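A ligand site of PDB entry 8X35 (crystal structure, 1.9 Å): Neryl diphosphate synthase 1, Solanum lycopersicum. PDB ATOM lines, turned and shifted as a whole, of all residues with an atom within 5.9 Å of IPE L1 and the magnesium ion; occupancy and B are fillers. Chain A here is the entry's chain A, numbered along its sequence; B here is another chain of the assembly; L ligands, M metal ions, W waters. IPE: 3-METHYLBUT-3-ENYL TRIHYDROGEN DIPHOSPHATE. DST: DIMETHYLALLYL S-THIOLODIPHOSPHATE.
An oxygen (O1B) of IPE L1 lies within hydrogen-bond range of the side-chain hydroxyl (OG) of Ser 259, 2.6 Å away.
O3B of IPE L1 is in hydrogen-bond range of N of Gly 301 of chain B.
O2B of IPE L1 lies within salt-bridge range of NH2 of Arg 257, 2.8 Å away.
O1A of IPE L1 is in hydrogen-bond range of ND2 of Asn 136, 3.1 Å away.
NH2 of Arg 251 lies within salt-bridge range of O2B of IPE L1, 3.4 Å away.
The backbone NH (N) of Phe 300 of chain B sits at hydrogen-bond distance from an oxygen (O3B) of IPE L1.
NH2 of Arg 139 lies within salt-bridge range of O1A of IPE L1 (3.6 Å).
The guanidinium group (NH2) of Arg 299 of chain B lies close to an oxygen (O5) of DST L2.
The guanidinium group of Arg 139 lies within salt-bridge range of an oxygen (O7) of DST L2, 2.7 Å away.
O4 of DST L2 sits at hydrogen-bond distance from N of Arg 92 (2.9 Å).
An oxygen (O4) of DST L2 lies within salt-bridge range of the guanidinium group (NE) of Arg 92.
N of Gly 89 sits close to S9 of DST L2.
An oxygen (O2) of DST L2 lies close to the backbone NH of Arg 91, at 3.1 Å.
The side-chain hydroxyl of Ser 259 sits at hydrogen-bond distance from the guanidinium group of Arg 251 (2.8 Å).
O of Gly 301 of chain B is in hydrogen-bond range of NE of Arg 139 (3.2 Å).
NH1 of Arg 251 sits at hydrogen-bond distance from O of Arg 257, at 2.8 Å.
The guanidinium group (NH2) of Arg 257 is in salt-bridge range of the side-chain carboxylate (OE1) of Glu 255, at 3.6 Å.
NH1 of Arg 257 sits at hydrogen-bond distance from O of His 297 of chain B, 3.0 Å away.
N of Ala 131 is in hydrogen-bond range of O of Ala 200.
The backbone NH of Phe 132 sits at hydrogen-bond distance from the backbone carbonyl oxygen of Ala 200 (3.3 Å).
The guanidinium group (NH2) of Arg 298 of chain B lies within hydrogen-bond range of the backbone carbonyl oxygen (O) of Tyr 268 of chain B.
Residues that only touch IPE L1: Arg 299 of chain B, Phe 130, Ala 131, Phe 132, Ile 86, Tyr 268 of chain B, Met 87 and Ser 133.
Along chain A the residues within 4 Å of IPE L1 span positions 86 to 259.
The nearest printed residue that does not touch IPE L1 is Glu 255 (4.4 Å).
NH2 of Arg 139 touches the magnesium ion (3.9 Å).
Two residues have an atom within 4 Å of the magnesium ion: Asp 88 and Arg 139.
The magnesium ion is bound by water W2, an oxygen (O2A) of IPE L1, the side-chain carboxylate (OD1) of Asp 88, an oxygen (O5) of DST L2, water W4 and an oxygen (O8) of DST L2.
Water W2 lies within hydrogen-bond range of an oxygen (O6) of DST L2, the guanidinium group of Arg 299 of chain B and the guanidinium group of Arg 139.
Water W4 lies within hydrogen-bond range of an oxygen (O2B) of IPE L1, the side-chain carboxylate of Asp 88 and the guanidinium group of Arg 299 of chain B.
Water W5 lies within hydrogen-bond range of an oxygen (O3B) of IPE L1 (2.8 Å), the guanidinium group (NH2) of Arg 139 (2.9 Å) and the backbone carbonyl oxygen (O) of Gly 302 of chain B (3.0 Å).
Water W3 lies within hydrogen-bond range of the side-chain hydroxyl (OG) of Ser 133 (2.7 Å), an oxygen (O1A) of IPE L1 (2.9 Å) and the side-chain hydroxyl (OH) of Tyr 268 of chain B (3.0 Å).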
ATOM      1  N   ILE A  86      15.037 -14.425  19.551  1.00  0.00           N
ATOM      2  CA  ILE A  86      13.910 -15.019  18.825  1.00  0.00           C
ATOM      3  C   ILE A  86      12.719 -15.099  19.781  1.00  0.00           C
ATOM      4  O   ILE A  86      12.739 -15.861  20.749  1.00  0.00           O
ATOM      5  CB  ILE A  86      14.257 -16.403  18.237  1.00  0.00           C
ATOM      6  CG1 ILE A  86      15.369 -16.266  17.180  1.00  0.00           C
ATOM      7  CG2 ILE A  86      13.010 -17.103  17.677  1.00  0.00           C
ATOM      8  CD1 ILE A  86      15.948 -17.632  16.705  1.00  0.00           C
ATOM      9  N   MET A  87      11.673 -14.309  19.503  1.00  0.00           N
ATOM     10  CA  MET A  87      10.587 -14.026  20.465  1.00  0.00           C
ATOM     11  C   MET A  87       9.411 -14.974  20.228  1.00  0.00           C
ATOM     12  O   MET A  87       8.369 -14.579  19.714  1.00  0.00           O
ATOM     13  CB  MET A  87      10.118 -12.572  20.311  1.00  0.00           C
ATOM     14  CG  MET A  87      11.186 -11.469  20.457  1.00  0.00           C
ATOM     15  SD  MET A  87      10.532  -9.753  20.312  1.00  0.00           S
ATOM     16  CE  MET A  87       9.986  -9.705  18.604  1.00  0.00           C
ATOM     17  N   ASP A  88       9.588 -16.238  20.623  1.00  0.00           N
ATOM     18  CA  ASP A  88       8.726 -17.338  20.214  1.00  0.00           C
ATOM     19  C   ASP A  88       7.847 -17.810  21.369  1.00  0.00           C
ATOM     20  O   ASP A  88       8.186 -17.684  22.556  1.00  0.00           O
ATOM     21  CB  ASP A  88       9.583 -18.515  19.691  1.00  0.00           C
ATOM     22  CG  ASP A  88       8.791 -19.574  18.925  1.00  0.00           C
ATOM     23  OD1 ASP A  88       7.731 -19.247  18.331  1.00  0.00           O
ATOM     24  OD2 ASP A  88       9.251 -20.746  18.870  1.00  0.00           O
ATOM     25  N   GLY A  89       6.701 -18.389  21.016  1.00  0.00           N
ATOM     26  CA  GLY A  89       5.835 -19.015  21.996  1.00  0.00           C
ATOM     27  C   GLY A  89       4.607 -18.219  22.422  1.00  0.00           C
ATOM     28  O   GLY A  89       4.008 -18.540  23.457  1.00  0.00           O
ATOM     29  N   ARG A  91       1.493 -17.740  20.956  1.00  0.00           N
ATOM     30  CA  ARG A  91       0.206 -18.419  20.834  1.00  0.00           C
ATOM     31  C   ARG A  91      -0.011 -19.451  21.930  1.00  0.00           C
ATOM     32  O   ARG A  91      -1.091 -19.498  22.549  1.00  0.00           O
ATOM     33  CB  ARG A  91       0.084 -19.093  19.478  1.00  0.00           C
ATOM     34  CG  ARG A  91       0.447 -18.207  18.341  1.00  0.00           C
ATOM     35  CD  ARG A  91       0.592 -18.966  17.032  1.00  0.00           C
ATOM     36  NE  ARG A  91      -0.672 -19.218  16.320  1.00  0.00           N
ATOM     37  CZ  ARG A  91      -1.627 -20.059  16.694  1.00  0.00           C
ATOM     38  NH1 ARG A  91      -1.476 -20.874  17.725  1.00  0.00           N
ATOM     39  NH2 ARG A  91      -2.749 -20.116  15.995  1.00  0.00           N
ATOM     40  N   ARG A  92       0.982 -20.310  22.151  1.00  0.00           N
ATOM     41  CA  ARG A  92       0.842 -21.322  23.189  1.00  0.00           C
ATOM     42  C   ARG A  92       0.599 -20.672  24.546  1.00  0.00           C
ATOM     43  O   ARG A  92      -0.180 -21.196  25.359  1.00  0.00           O
ATOM     44  CB  ARG A  92       2.083 -22.223  23.219  1.00  0.00           C
ATOM     45  CG  ARG A  92       2.103 -23.280  22.094  1.00  0.00           C
ATOM     46  CD  ARG A  92       3.499 -23.944  21.923  1.00  0.00           C
ATOM     47  NE  ARG A  92       4.447 -23.042  21.267  1.00  0.00           N
ATOM     48  CZ  ARG A  92       5.766 -23.139  21.372  1.00  0.00           C
ATOM     49  NH1 ARG A  92       6.343 -24.056  22.129  1.00  0.00           N
ATOM     50  NH2 ARG A  92       6.522 -22.307  20.661  1.00  0.00           N
ATOM     51  N   PHE A 130      13.695 -10.858  16.448  1.00  0.00           N
ATOM     52  CA  PHE A 130      12.969 -11.450  15.315  1.00  0.00           C
ATOM     53  C   PHE A 130      11.479 -11.260  15.571  1.00  0.00           C
ATOM     54  O   PHE A 130      10.902 -11.929  16.441  1.00  0.00           O
ATOM     55  CB  PHE A 130      13.348 -12.929  15.183  1.00  0.00           C
ATOM     56  CG  PHE A 130      13.272 -13.494  13.764  1.00  0.00           C
ATOM     57  CD1 PHE A 130      13.066 -12.665  12.665  1.00  0.00           C
ATOM     58  CD2 PHE A 130      13.504 -14.852  13.547  1.00  0.00           C
ATOM     59  CE1 PHE A 130      13.023 -13.207  11.356  1.00  0.00           C
ATOM     60  CE2 PHE A 130      13.507 -15.395  12.241  1.00  0.00           C
ATOM     61  CZ  PHE A 130      13.270 -14.583  11.148  1.00  0.00           C
ATOM     62  N   ALA A 131      10.826 -10.360  14.817  1.00  0.00           N
ATOM     63  CA  ALA A 131       9.406 -10.096  15.013  1.00  0.00           C
ATOM     64  C   ALA A 131       8.509 -10.739  13.963  1.00  0.00           C
ATOM     65  O   ALA A 131       7.353 -11.043  14.279  1.00  0.00           O
ATOM     66  CB  ALA A 131       9.135  -8.583  15.012  1.00  0.00           C
ATOM     67  N   PHE A 132       8.970 -10.906  12.721  1.00  0.00           N
ATOM     68  CA  PHE A 132       8.162 -11.472  11.642  1.00  0.00           C
ATOM     69  C   PHE A 132       9.105 -12.020  10.578  1.00  0.00           C
ATOM     70  O   PHE A 132       9.898 -11.262   9.994  1.00  0.00           O
ATOM     71  CB  PHE A 132       7.223 -10.399  11.032  1.00  0.00           C
ATOM     72  CG  PHE A 132       6.119 -10.979  10.172  1.00  0.00           C
ATOM     73  CD1 PHE A 132       4.911 -11.367  10.742  1.00  0.00           C
ATOM     74  CD2 PHE A 132       6.297 -11.126   8.796  1.00  0.00           C
ATOM     75  CE1 PHE A 132       3.897 -11.911   9.958  1.00  0.00           C
ATOM     76  CE2 PHE A 132       5.282 -11.658   8.006  1.00  0.00           C
ATOM     77  CZ  PHE A 132       4.084 -12.055   8.586  1.00  0.00           C
ATOM     78  N   SER A 133       9.042 -13.336  10.334  1.00  0.00           N
ATOM     79  CA  SER A 133       9.933 -13.944   9.353  1.00  0.00           C
ATOM     80  C   SER A 133       9.283 -13.990   7.968  1.00  0.00           C
ATOM     81  O   SER A 133       8.062 -13.833   7.829  1.00  0.00           O
ATOM     82  CB  SER A 133      10.326 -15.369   9.768  1.00  0.00           C
ATOM     83  OG  SER A 133       9.345 -16.288   9.366  1.00  0.00           O
ATOM     84  N   ASN A 136       6.479 -16.516   7.819  1.00  0.00           N
ATOM     85  CA  ASN A 136       5.234 -16.304   8.578  1.00  0.00           C
ATOM     86  C   ASN A 136       4.067 -15.840   7.705  1.00  0.00           C
ATOM     87  O   ASN A 136       2.930 -15.788   8.191  1.00  0.00           O
ATOM     88  CB  ASN A 136       5.448 -15.279   9.705  1.00  0.00           C
ATOM     89  CG  ASN A 136       6.334 -15.783  10.836  1.00  0.00           C
ATOM     90  OD1 ASN A 136       7.047 -14.991  11.463  1.00  0.00           O
ATOM     91  ND2 ASN A 136       6.294 -17.103  11.118  1.00  0.00           N
ATOM     92  N   ARG A 139       0.809 -18.128   7.484  1.00  0.00           N
ATOM     93  CA  ARG A 139      -0.278 -18.215   8.446  1.00  0.00           C
ATOM     94  C   ARG A 139      -1.570 -17.655   7.836  1.00  0.00           C
ATOM     95  O   ARG A 139      -1.593 -17.152   6.710  1.00  0.00           O
ATOM     96  CB  ARG A 139       0.126 -17.495   9.738  1.00  0.00           C
ATOM     97  CG  ARG A 139       1.450 -18.014  10.298  1.00  0.00           C
ATOM     98  CD  ARG A 139       1.848 -17.359  11.605  1.00  0.00           C
ATOM     99  NE  ARG A 139       2.979 -18.063  12.229  1.00  0.00           N
ATOM    100  CZ  ARG A 139       3.371 -17.917  13.487  1.00  0.00           C
ATOM    101  NH1 ARG A 139       2.717 -17.116  14.329  1.00  0.00           N
ATOM    102  NH2 ARG A 139       4.441 -18.586  13.914  1.00  0.00           N
ATOM    103  N   ALA A 200      13.765  -7.079  13.250  1.00  0.00           N
ATOM    104  CA  ALA A 200      13.762  -7.810  11.986  1.00  0.00           C
ATOM    105  C   ALA A 200      12.311  -8.140  11.635  1.00  0.00           C
ATOM    106  O   ALA A 200      11.685  -8.993  12.287  1.00  0.00           O
ATOM    107  CB  ALA A 200      14.605  -9.089  12.071  1.00  0.00           C
ATOM    108  N   ARG A 251      16.616 -17.906  22.481  1.00  0.00           N
ATOM    109  CA  ARG A 251      15.338 -18.258  21.857  1.00  0.00           C
ATOM    110  C   ARG A 251      14.398 -18.815  22.912  1.00  0.00           C
ATOM    111  O   ARG A 251      14.650 -19.881  23.483  1.00  0.00           O
ATOM    112  CB  ARG A 251      15.504 -19.269  20.706  1.00  0.00           C
ATOM    113  CG  ARG A 251      14.144 -19.769  20.174  1.00  0.00           C
ATOM    114  CD  ARG A 251      14.245 -20.597  18.867  1.00  0.00           C
ATOM    115  NE  ARG A 251      12.926 -20.896  18.310  1.00  0.00           N
ATOM    116  CZ  ARG A 251      12.645 -20.988  17.019  1.00  0.00           C
ATOM    117  NH1 ARG A 251      13.581 -20.861  16.095  1.00  0.00           N
ATOM    118  NH2 ARG A 251      11.387 -21.214  16.647  1.00  0.00           N
ATOM    119  N   GLU A 255      11.751 -24.429  21.296  1.00  0.00           N
ATOM    120  CA  GLU A 255      12.253 -25.080  20.086  1.00  0.00           C
ATOM    121  C   GLU A 255      13.746 -24.822  19.933  1.00  0.00           C
ATOM    122  O   GLU A 255      14.262 -23.773  20.349  1.00  0.00           O
ATOM    123  CB  GLU A 255      11.490 -24.589  18.851  1.00  0.00           C
ATOM    124  CG  GLU A 255       9.967 -24.552  19.053  1.00  0.00           C
ATOM    125  CD  GLU A 255       9.351 -25.937  19.220  1.00  0.00           C
ATOM    126  OE1 GLU A 255      10.033 -26.935  18.900  1.00  0.00           O
ATOM    127  OE2 GLU A 255       8.209 -26.020  19.726  1.00  0.00           O
ATOM    128  N   ARG A 257      16.275 -24.565  17.136  1.00  0.00           N
ATOM    129  CA  ARG A 257      16.436 -24.304  15.714  1.00  0.00           C
ATOM    130  C   ARG A 257      16.465 -22.785  15.571  1.00  0.00           C
ATOM    131  O   ARG A 257      16.024 -22.060  16.493  1.00  0.00           O
ATOM    132  CB  ARG A 257      15.292 -24.930  14.901  1.00  0.00           C
ATOM    133  CG  ARG A 257      13.868 -24.647  15.488  1.00  0.00           C
ATOM    134  CD  ARG A 257      12.808 -25.134  14.534  1.00  0.00           C
ATOM    135  NE  ARG A 257      11.455 -24.929  15.031  1.00  0.00           N
ATOM    136  CZ  ARG A 257      10.600 -25.887  15.386  1.00  0.00           C
ATOM    137  NH1 ARG A 257      10.969 -27.168  15.437  1.00  0.00           N
ATOM    138  NH2 ARG A 257       9.350 -25.554  15.686  1.00  0.00           N
ATOM    139  N   VAL A 258      17.014 -22.296  14.458  1.00  0.00           N
ATOM    140  CA  VAL A 258      17.139 -20.845  14.236  1.00  0.00           C
ATOM    141  C   VAL A 258      16.070 -20.272  13.315  1.00  0.00           C
ATOM    142  O   VAL A 258      15.906 -19.037  13.263  1.00  0.00           O
ATOM    143  CB  VAL A 258      18.554 -20.482  13.720  1.00  0.00           C
ATOM    144  CG1 VAL A 258      19.585 -20.845  14.775  1.00  0.00           C
ATOM    145  CG2 VAL A 258      18.891 -21.121  12.328  1.00  0.00           C
ATOM    146  N   SER A 259      15.308 -21.112  12.607  1.00  0.00           N
ATOM    147  CA  SER A 259      14.134 -20.684  11.852  1.00  0.00           C
ATOM    148  C   SER A 259      14.446 -19.534  10.881  1.00  0.00           C
ATOM    149  O   SER A 259      13.742 -18.519  10.839  1.00  0.00           O
ATOM    150  CB  SER A 259      12.990 -20.301  12.806  1.00  0.00           C
ATOM    151  OG  SER A 259      12.566 -21.429  13.572  1.00  0.00           O
ATOM    152  N   TYR B 268      16.420 -24.384   8.890  1.00  0.00           N
ATOM    153  CA  TYR B 268      15.369 -25.029   9.681  1.00  0.00           C
ATOM    154  C   TYR B 268      15.786 -26.415  10.211  1.00  0.00           C
ATOM    155  O   TYR B 268      14.929 -27.221  10.596  1.00  0.00           O
ATOM    156  CB  TYR B 268      14.049 -25.111   8.877  1.00  0.00           C
ATOM    157  CG  TYR B 268      13.268 -23.764   8.829  1.00  0.00           C
ATOM    158  CD1 TYR B 268      12.358 -23.429   9.846  1.00  0.00           C
ATOM    159  CD2 TYR B 268      13.452 -22.847   7.798  1.00  0.00           C
ATOM    160  CE1 TYR B 268      11.660 -22.193   9.810  1.00  0.00           C
ATOM    161  CE2 TYR B 268      12.767 -21.637   7.755  1.00  0.00           C
ATOM    162  CZ  TYR B 268      11.865 -21.307   8.760  1.00  0.00           C
ATOM    163  OH  TYR B 268      11.193 -20.065   8.712  1.00  0.00           O
ATOM    164  N   HIS B 297       8.316 -31.065  17.042  1.00  0.00           N
ATOM    165  CA  HIS B 297       7.301 -30.629  16.091  1.00  0.00           C
ATOM    166  C   HIS B 297       7.869 -29.517  15.227  1.00  0.00           C
ATOM    167  O   HIS B 297       8.238 -28.440  15.735  1.00  0.00           O
ATOM    168  CB  HIS B 297       6.030 -30.148  16.787  1.00  0.00           C
ATOM    169  CG  HIS B 297       5.414 -31.186  17.668  1.00  0.00           C
ATOM    170  ND1 HIS B 297       5.621 -31.209  19.033  1.00  0.00           N
ATOM    171  CD2 HIS B 297       4.617 -32.238  17.378  1.00  0.00           C
ATOM    172  CE1 HIS B 297       4.968 -32.245  19.542  1.00  0.00           C
ATOM    173  NE2 HIS B 297       4.362 -32.889  18.570  1.00  0.00           N
ATOM    174  N   ARG B 298       7.935 -29.763  13.921  1.00  0.00           N
ATOM    175  CA  ARG B 298       8.526 -28.825  12.978  1.00  0.00           C
ATOM    176  C   ARG B 298       7.406 -28.041  12.291  1.00  0.00           C
ATOM    177  O   ARG B 298       6.515 -28.642  11.691  1.00  0.00           O
ATOM    178  CB  ARG B 298       9.391 -29.578  11.972  1.00  0.00           C
ATOM    179  CG  ARG B 298      10.502 -30.386  12.647  1.00  0.00           C
ATOM    180  CD  ARG B 298      11.374 -31.164  11.621  1.00  0.00           C
ATOM    181  NE  ARG B 298      12.386 -30.326  10.981  1.00  0.00           N
ATOM    182  CZ  ARG B 298      13.122 -30.696   9.940  1.00  0.00           C
ATOM    183  NH1 ARG B 298      12.965 -31.877   9.364  1.00  0.00           N
ATOM    184  NH2 ARG B 298      14.054 -29.865   9.476  1.00  0.00           N
ATOM    185  N   ARG B 299       7.459 -26.717  12.400  1.00  0.00           N
ATOM    186  CA  ARG B 299       6.394 -25.826  11.933  1.00  0.00           C
ATOM    187  C   ARG B 299       6.783 -24.997  10.712  1.00  0.00           C
ATOM    188  O   ARG B 299       5.891 -24.527   9.994  1.00  0.00           O
ATOM    189  CB  ARG B 299       5.960 -24.920  13.092  1.00  0.00           C
ATOM    190  CG  ARG B 299       5.226 -25.735  14.168  1.00  0.00           C
ATOM    191  CD  ARG B 299       4.232 -24.896  14.956  1.00  0.00           C
ATOM    192  NE  ARG B 299       4.879 -24.297  16.125  1.00  0.00           N
ATOM    193  CZ  ARG B 299       5.461 -24.984  17.106  1.00  0.00           C
ATOM    194  NH1 ARG B 299       5.277 -26.290  17.236  1.00  0.00           N
ATOM    195  NH2 ARG B 299       6.216 -24.360  18.003  1.00  0.00           N
ATOM    196  N   PHE B 300       8.078 -24.822  10.451  1.00  0.00           N
ATOM    197  CA  PHE B 300       8.560 -24.133   9.244  1.00  0.00           C
ATOM    198  C   PHE B 300       7.883 -22.764   9.057  1.00  0.00           C
ATOM    199  O   PHE B 300       7.667 -22.316   7.939  1.00  0.00           O
ATOM    200  CB  PHE B 300       8.366 -25.001   7.998  1.00  0.00           C
ATOM    201  CG  PHE B 300       9.055 -26.343   8.065  1.00  0.00           C
ATOM    202  CD1 PHE B 300      10.448 -26.448   7.997  1.00  0.00           C
ATOM    203  CD2 PHE B 300       8.319 -27.506   8.210  1.00  0.00           C
ATOM    204  CE1 PHE B 300      11.079 -27.669   8.064  1.00  0.00           C
ATOM    205  CE2 PHE B 300       8.962 -28.770   8.285  1.00  0.00           C
ATOM    206  CZ  PHE B 300      10.342 -28.832   8.209  1.00  0.00           C
ATOM    207  N   GLY B 301       7.516 -22.099  10.168  1.00  0.00           N
ATOM    208  CA  GLY B 301       6.939 -20.768  10.096  1.00  0.00           C
ATOM    209  C   GLY B 301       5.420 -20.712  10.025  1.00  0.00           C
ATOM    210  O   GLY B 301       4.848 -19.615  10.183  1.00  0.00           O
ATOM    211  N   GLY B 302       4.750 -21.847   9.807  1.00  0.00           N
ATOM    212  CA  GLY B 302       3.303 -21.881   9.731  1.00  0.00           C
ATOM    213  C   GLY B 302       2.643 -22.540  10.919  1.00  0.00           C
ATOM    214  O   GLY B 302       3.123 -22.407  12.051  1.00  0.00           O
ATOM    215  N   HIS B 303       1.546 -23.262  10.679  1.00  0.00           N
ATOM    216  CA  HIS B 303       0.864 -24.013  11.741  1.00  0.00           C
ATOM    217  C   HIS B 303       0.319 -25.343  11.240  1.00  0.00           C
ATOM    218  O   HIS B 303       0.550 -26.394  11.845  1.00  0.00           O
ATOM    219  CB  HIS B 303      -0.272 -23.169  12.329  1.00  0.00           C
ATOM    220  CG  HIS B 303       0.219 -22.021  13.142  1.00  0.00           C
ATOM    221  ND1 HIS B 303       0.055 -20.705  12.751  1.00  0.00           N
ATOM    222  CD2 HIS B 303       0.903 -21.980  14.310  1.00  0.00           C
ATOM    223  CE1 HIS B 303       0.602 -19.912  13.655  1.00  0.00           C
ATOM    224  NE2 HIS B 303       1.130 -20.664  14.604  1.00  0.00           N
HETATM  225  C1  IPE L   1      10.487 -17.792  14.309  1.00  0.00           C
HETATM  226  O1  IPE L   1       9.409 -18.340  15.030  1.00  0.00           O
HETATM  227  C2  IPE L   1      10.060 -16.475  13.633  1.00  0.00           C
HETATM  228  C3  IPE L   1       9.882 -15.337  14.632  1.00  0.00           C
HETATM  229  C4  IPE L   1       9.529 -14.117  14.198  1.00  0.00           C
HETATM  230  C5  IPE L   1      10.110 -15.547  16.127  1.00  0.00           C
HETATM  231  PA  IPE L   1       8.457 -19.485  14.326  1.00  0.00           P
HETATM  232  O1A IPE L   1       7.933 -18.974  12.992  1.00  0.00           O
HETATM  233  O2A IPE L   1       7.331 -19.896  15.261  1.00  0.00           O
HETATM  234  O3A IPE L   1       9.518 -20.698  14.020  1.00  0.00           O
HETATM  235  PB  IPE L   1       9.146 -22.262  13.812  1.00  0.00           P
HETATM  236  O1B IPE L   1      10.424 -22.845  13.209  1.00  0.00           O
HETATM  237  O2B IPE L   1       8.806 -22.895  15.120  1.00  0.00           O
HETATM  238  O3B IPE L   1       8.029 -22.398  12.821  1.00  0.00           O
HETATM  239  O4  DST L   2       3.297 -20.643  20.358  1.00  0.00           O
HETATM  240  P1  DST L   2       3.721 -20.322  18.952  1.00  0.00           P
HETATM  241  O6  DST L   2       2.872 -21.122  17.975  1.00  0.00           O
HETATM  242  O5  DST L   2       5.215 -20.574  18.762  1.00  0.00           O
HETATM  243  O2  DST L   2       3.446 -18.720  18.740  1.00  0.00           O
HETATM  244  P3  DST L   2       4.136 -17.744  17.630  1.00  0.00           P
HETATM  245  O8  DST L   2       4.856 -18.507  16.518  1.00  0.00           O
HETATM  246  O7  DST L   2       3.102 -16.849  16.994  1.00  0.00           O
HETATM  247  S9  DST L   2       5.620 -16.598  18.567  1.00  0.00           S
HETATM  248  C10 DST L   2       6.725 -15.809  17.346  1.00  0.00           C
HETATM  249  C11 DST L   2       6.074 -14.489  16.920  1.00  0.00           C
HETATM  250  C12 DST L   2       5.804 -14.269  15.653  1.00  0.00           C
HETATM  251  C13 DST L   2       5.142 -12.956  15.231  1.00  0.00           C
HETATM  252  C14 DST L   2       6.132 -15.312  14.583  1.00  0.00           C
HETATM  253 MG    MG M   1       6.338 -20.166  16.943  1.00  0.00          MG
HETATM  254  O   HOH W   1      10.295 -25.491  12.340  1.00  0.00           O
HETATM  255  O   HOH W   2       5.057 -21.238  15.987  1.00  0.00           O
HETATM  256  O   HOH W   3       9.780 -18.485  10.786  1.00  0.00           O
HETATM  257  O   HOH W   4       7.600 -21.976  17.212  1.00  0.00           O
HETATM  258  O   HOH W   5       5.553 -21.213  13.300  1.00  0.00           O
